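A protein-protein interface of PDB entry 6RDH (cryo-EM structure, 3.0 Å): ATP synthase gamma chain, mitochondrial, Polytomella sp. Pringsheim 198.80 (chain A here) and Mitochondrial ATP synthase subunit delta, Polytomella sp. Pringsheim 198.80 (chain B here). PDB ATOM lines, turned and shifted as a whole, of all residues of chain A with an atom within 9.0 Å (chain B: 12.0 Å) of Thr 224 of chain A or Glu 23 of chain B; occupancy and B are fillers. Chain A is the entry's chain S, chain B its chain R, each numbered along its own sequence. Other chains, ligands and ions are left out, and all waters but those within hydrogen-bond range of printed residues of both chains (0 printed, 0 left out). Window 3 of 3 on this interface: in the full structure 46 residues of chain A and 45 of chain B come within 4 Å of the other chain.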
ATOM      1  N   LEU A 216     -29.952 -12.078   4.759  1.00  0.00           N
ATOM      2  CA  LEU A 216     -28.797 -12.955   4.653  1.00  0.00           C
ATOM      3  C   LEU A 216     -28.529 -13.450   3.242  1.00  0.00           C
ATOM      4  O   LEU A 216     -27.381 -13.791   2.942  1.00  0.00           O
ATOM      5  CB  LEU A 216     -28.982 -14.150   5.592  1.00  0.00           C
ATOM      6  CG  LEU A 216     -27.808 -15.044   5.975  1.00  0.00           C
ATOM      7  CD1 LEU A 216     -26.782 -14.248   6.735  1.00  0.00           C
ATOM      8  CD2 LEU A 216     -28.319 -16.161   6.832  1.00  0.00           C
ATOM      9  N   GLU A 217     -29.527 -13.467   2.354  1.00  0.00           N
ATOM     10  CA  GLU A 217     -29.378 -14.119   1.057  1.00  0.00           C
ATOM     11  C   GLU A 217     -28.507 -13.300   0.118  1.00  0.00           C
ATOM     12  O   GLU A 217     -27.635 -13.850  -0.563  1.00  0.00           O
ATOM     13  CB  GLU A 217     -30.756 -14.358   0.441  1.00  0.00           C
ATOM     14  CG  GLU A 217     -30.788 -14.558  -1.035  1.00  0.00           C
ATOM     15  CD  GLU A 217     -30.154 -15.846  -1.415  1.00  0.00           C
ATOM     16  OE1 GLU A 217     -30.443 -16.856  -0.749  1.00  0.00           O
ATOM     17  OE2 GLU A 217     -29.359 -15.855  -2.365  1.00  0.00           O
ATOM     18  N   LYS A 218     -28.728 -11.988   0.071  1.00  0.00           N
ATOM     19  CA  LYS A 218     -27.880 -11.129  -0.743  1.00  0.00           C
ATOM     20  C   LYS A 218     -26.481 -11.024  -0.153  1.00  0.00           C
ATOM     21  O   LYS A 218     -25.511 -10.866  -0.897  1.00  0.00           O
ATOM     22  CB  LYS A 218     -28.533  -9.753  -0.880  1.00  0.00           C
ATOM     23  CG  LYS A 218     -27.925  -8.824  -1.920  1.00  0.00           C
ATOM     24  CD  LYS A 218     -26.960  -7.816  -1.311  1.00  0.00           C
ATOM     25  CE  LYS A 218     -26.405  -6.880  -2.362  1.00  0.00           C
ATOM     26  NZ  LYS A 218     -25.449  -5.904  -1.791  1.00  0.00           N
ATOM     27  N   GLN A 219     -26.359 -11.130   1.170  1.00  0.00           N
ATOM     28  CA  GLN A 219     -25.050 -11.081   1.808  1.00  0.00           C
ATOM     29  C   GLN A 219     -24.255 -12.349   1.549  1.00  0.00           C
ATOM     30  O   GLN A 219     -23.024 -12.307   1.494  1.00  0.00           O
ATOM     31  CB  GLN A 219     -25.207 -10.834   3.301  1.00  0.00           C
ATOM     32  CG  GLN A 219     -25.816  -9.485   3.606  1.00  0.00           C
ATOM     33  CD  GLN A 219     -25.882  -9.175   5.086  1.00  0.00           C
ATOM     34  OE1 GLN A 219     -25.402  -9.944   5.919  1.00  0.00           O
ATOM     35  NE2 GLN A 219     -26.489  -8.043   5.424  1.00  0.00           N
ATOM     36  N   LEU A 220     -24.930 -13.476   1.384  1.00  0.00           N
ATOM     37  CA  LEU A 220     -24.249 -14.708   1.021  1.00  0.00           C
ATOM     38  C   LEU A 220     -23.978 -14.824  -0.468  1.00  0.00           C
ATOM     39  O   LEU A 220     -23.208 -15.701  -0.871  1.00  0.00           O
ATOM     40  CB  LEU A 220     -25.055 -15.923   1.480  1.00  0.00           C
ATOM     41  CG  LEU A 220     -24.633 -16.610   2.781  1.00  0.00           C
ATOM     42  CD1 LEU A 220     -23.283 -17.233   2.554  1.00  0.00           C
ATOM     43  CD2 LEU A 220     -24.587 -15.673   3.970  1.00  0.00           C
ATOM     44  N   GLU A 221     -24.597 -13.990  -1.295  1.00  0.00           N
ATOM     45  CA  GLU A 221     -24.324 -14.060  -2.721  1.00  0.00           C
ATOM     46  C   GLU A 221     -23.227 -13.118  -3.183  1.00  0.00           C
ATOM     47  O   GLU A 221     -22.683 -13.331  -4.270  1.00  0.00           O
ATOM     48  CB  GLU A 221     -25.593 -13.788  -3.519  1.00  0.00           C
ATOM     49  CG  GLU A 221     -26.486 -14.984  -3.602  1.00  0.00           C
ATOM     50  CD  GLU A 221     -26.067 -15.916  -4.717  1.00  0.00           C
ATOM     51  OE1 GLU A 221     -25.861 -15.437  -5.850  1.00  0.00           O
ATOM     52  OE2 GLU A 221     -25.911 -17.126  -4.456  1.00  0.00           O
ATOM     53  N   ASP A 222     -22.882 -12.091  -2.413  1.00  0.00           N
ATOM     54  CA  ASP A 222     -21.860 -11.157  -2.883  1.00  0.00           C
ATOM     55  C   ASP A 222     -20.485 -11.741  -2.589  1.00  0.00           C
ATOM     56  O   ASP A 222     -20.160 -12.118  -1.466  1.00  0.00           O
ATOM     57  CB  ASP A 222     -22.066  -9.743  -2.332  1.00  0.00           C
ATOM     58  CG  ASP A 222     -22.092  -9.659  -0.824  1.00  0.00           C
ATOM     59  OD1 ASP A 222     -21.057  -9.834  -0.172  1.00  0.00           O
ATOM     60  OD2 ASP A 222     -23.162  -9.333  -0.285  1.00  0.00           O
ATOM     61  N   VAL A 223     -19.723 -11.954  -3.656  1.00  0.00           N
ATOM     62  CA  VAL A 223     -18.308 -12.300  -3.568  1.00  0.00           C
ATOM     63  C   VAL A 223     -17.561 -11.215  -4.333  1.00  0.00           C
ATOM     64  O   VAL A 223     -17.375 -11.328  -5.554  1.00  0.00           O
ATOM     65  CB  VAL A 223     -18.008 -13.698  -4.123  1.00  0.00           C
ATOM     66  CG1 VAL A 223     -16.543 -14.055  -3.928  1.00  0.00           C
ATOM     67  CG2 VAL A 223     -18.888 -14.749  -3.441  1.00  0.00           C
ATOM     68  N   THR A 224     -17.143 -10.167  -3.610  1.00  0.00           N
ATOM     69  CA  THR A 224     -16.417  -8.996  -4.120  1.00  0.00           C
ATOM     70  C   THR A 224     -17.175  -8.348  -5.287  1.00  0.00           C
ATOM     71  O   THR A 224     -16.779  -8.408  -6.454  1.00  0.00           O
ATOM     72  CB  THR A 224     -14.974  -9.366  -4.494  1.00  0.00           C
ATOM     73  OG1 THR A 224     -14.402 -10.134  -3.430  1.00  0.00           O
ATOM     74  CG2 THR A 224     -14.126  -8.110  -4.642  1.00  0.00           C
ATOM     75  N   GLY A 225     -18.317  -7.758  -4.944  1.00  0.00           N
ATOM     76  CA  GLY A 225     -19.289  -7.326  -5.931  1.00  0.00           C
ATOM     77  C   GLY A 225     -20.636  -7.960  -5.654  1.00  0.00           C
ATOM     78  O   GLY A 225     -21.265  -7.620  -4.649  1.00  0.00           O
ATOM     79  N   ASN A 226     -21.086  -8.847  -6.548  1.00  0.00           N
ATOM     80  CA  ASN A 226     -22.166  -9.799  -6.291  1.00  0.00           C
ATOM     81  C   ASN A 226     -22.184 -10.853  -7.385  1.00  0.00           C
ATOM     82  O   ASN A 226     -21.651 -10.659  -8.478  1.00  0.00           O
ATOM     83  CB  ASN A 226     -23.547  -9.143  -6.211  1.00  0.00           C
ATOM     84  CG  ASN A 226     -24.511  -9.922  -5.346  1.00  0.00           C
ATOM     85  OD1 ASN A 226     -24.542 -11.147  -5.390  1.00  0.00           O
ATOM     86  ND2 ASN A 226     -25.298  -9.215  -4.552  1.00  0.00           N
ATOM     87  N   SER A 227     -22.802 -11.985  -7.057  1.00  0.00           N
ATOM     88  CA  SER A 227     -23.217 -12.972  -8.040  1.00  0.00           C
ATOM     89  C   SER A 227     -24.668 -12.790  -8.448  1.00  0.00           C
ATOM     90  O   SER A 227     -25.105 -13.395  -9.430  1.00  0.00           O
ATOM     91  CB  SER A 227     -23.021 -14.384  -7.487  1.00  0.00           C
ATOM     92  OG  SER A 227     -23.613 -14.498  -6.205  1.00  0.00           O
ATOM     93  N   ASP A 229     -25.841  -9.568  -8.986  1.00  0.00           N
ATOM     94  CA  ASP A 229     -25.863  -8.388  -9.837  1.00  0.00           C
ATOM     95  C   ASP A 229     -25.553  -8.696 -11.292  1.00  0.00           C
ATOM     96  O   ASP A 229     -25.482  -7.768 -12.099  1.00  0.00           O
ATOM     97  CB  ASP A 229     -24.894  -7.329  -9.311  1.00  0.00           C
ATOM     98  CG  ASP A 229     -25.512  -6.473  -8.218  1.00  0.00           C
ATOM     99  OD1 ASP A 229     -24.956  -6.400  -7.105  1.00  0.00           O
ATOM    100  OD2 ASP A 229     -26.580  -5.877  -8.468  1.00  0.00           O
ATOM    101  N   GLU B  23     -17.252  -9.552   3.285  1.00  0.00           N
ATOM    102  CA  GLU B  23     -18.490  -9.456   2.522  1.00  0.00           C
ATOM    103  C   GLU B  23     -19.262 -10.778   2.528  1.00  0.00           C
ATOM    104  O   GLU B  23     -20.493 -10.790   2.497  1.00  0.00           O
ATOM    105  CB  GLU B  23     -18.195  -9.012   1.086  1.00  0.00           C
ATOM    106  CG  GLU B  23     -17.026  -9.715   0.422  1.00  0.00           C
ATOM    107  CD  GLU B  23     -15.750  -8.900   0.494  1.00  0.00           C
ATOM    108  OE1 GLU B  23     -15.758  -7.850   1.169  1.00  0.00           O
ATOM    109  OE2 GLU B  23     -14.742  -9.305  -0.123  1.00  0.00           O
ATOM    110  N   ALA B  24     -18.526 -11.886   2.592  1.00  0.00           N
ATOM    111  CA  ALA B  24     -19.110 -13.223   2.585  1.00  0.00           C
ATOM    112  C   ALA B  24     -18.744 -13.940   3.875  1.00  0.00           C
ATOM    113  O   ALA B  24     -18.272 -15.082   3.847  1.00  0.00           O
ATOM    114  CB  ALA B  24     -18.640 -14.021   1.369  1.00  0.00           C
ATOM    115  N   ALA B  25     -18.971 -13.265   5.012  1.00  0.00           N
ATOM    116  CA  ALA B  25     -18.440 -13.629   6.327  1.00  0.00           C
ATOM    117  C   ALA B  25     -18.882 -15.001   6.833  1.00  0.00           C
ATOM    118  O   ALA B  25     -18.321 -15.482   7.824  1.00  0.00           O
ATOM    119  CB  ALA B  25     -18.835 -12.563   7.353  1.00  0.00           C
ATOM    120  N   ALA B  26     -19.860 -15.641   6.194  1.00  0.00           N
ATOM    121  CA  ALA B  26     -20.241 -17.014   6.501  1.00  0.00           C
ATOM    122  C   ALA B  26     -19.929 -17.884   5.291  1.00  0.00           C
ATOM    123  O   ALA B  26     -20.772 -18.026   4.397  1.00  0.00           O
ATOM    124  CB  ALA B  26     -21.727 -17.093   6.858  1.00  0.00           C
ATOM    125  N   PRO B  27     -18.740 -18.492   5.206  1.00  0.00           N
ATOM    126  CA  PRO B  27     -18.436 -19.352   4.050  1.00  0.00           C
ATOM    127  C   PRO B  27     -19.224 -20.651   4.077  1.00  0.00           C
ATOM    128  O   PRO B  27     -18.706 -21.707   4.448  1.00  0.00           O
ATOM    129  CB  PRO B  27     -16.930 -19.607   4.181  1.00  0.00           C
ATOM    130  CG  PRO B  27     -16.436 -18.556   5.116  1.00  0.00           C
ATOM    131  CD  PRO B  27     -17.560 -18.278   6.054  1.00  0.00           C
ATOM    132  N   ALA B  28     -20.487 -20.567   3.667  1.00  0.00           N
ATOM    133  CA  ALA B  28     -21.425 -21.674   3.757  1.00  0.00           C
ATOM    134  C   ALA B  28     -21.248 -22.603   2.564  1.00  0.00           C
ATOM    135  O   ALA B  28     -20.299 -22.487   1.784  1.00  0.00           O
ATOM    136  CB  ALA B  28     -22.850 -21.144   3.836  1.00  0.00           C
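Of the printed residues of chain B, Thr 224 of chain A touches Glu 23 (3.4 Å).
Glu 23 of chain B touches three residues of chain A.
Gln 219 of chain A touches just one residue of chain B: Glu 23 (3.1 Å).
Asp 222 of chain A touches just these residues of chain B: Glu 23 and Ala 24.
No residue of chain B comes within 4 Å of Val 223 of chain A.
No residue of chain B comes within 4 Å of Gly 225 of chain A.
Of the printed residues of chain A, Ala 26 of chain B touches Leu 220.
Asn 226 of chain A touches none of the printed residues of chain B.
Ser 227 of chain A touches none of the printed residues of chain B.
The nearest residue of chain A that does not touch Glu 23 of chain B is Val 223 of chain A (4.9 Å).
The nearest printed residue of chain A that does not touch Ala 26 of chain B is Leu 216 of chain A (5.8 Å).
Ala 26 of chain B touches Leu 220 of chain A (O to CD1, 3.2 Å).
Asp 222 of chain A touches Ala 24 of chain B.
O of Glu 23 of chain B lies close to OD1 of Asp 222 of chain A.
The backbone carbonyl oxygen (O) of Glu 23 of chain B sits close to the backbone carbonyl oxygen (O) of Gln 219 of chain A, 3.1 Å away.
OG1 of Thr 224 of chain A sits at hydrogen-bond distance from OE2 of Glu 23 of chain B (3.4 Å).
Of the 13 printed residues of chain A, 4 touch a printed residue of chain B.
Printed residues of chain A that touch a printed residue of chain B: Gln 219, Leu 220, Asp 222 and Thr 224.
Along chain A the printed residues that touch a printed residue of chain B span positions 219 to 224.
Among the printed residues, 5 pairs touch across the chains.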
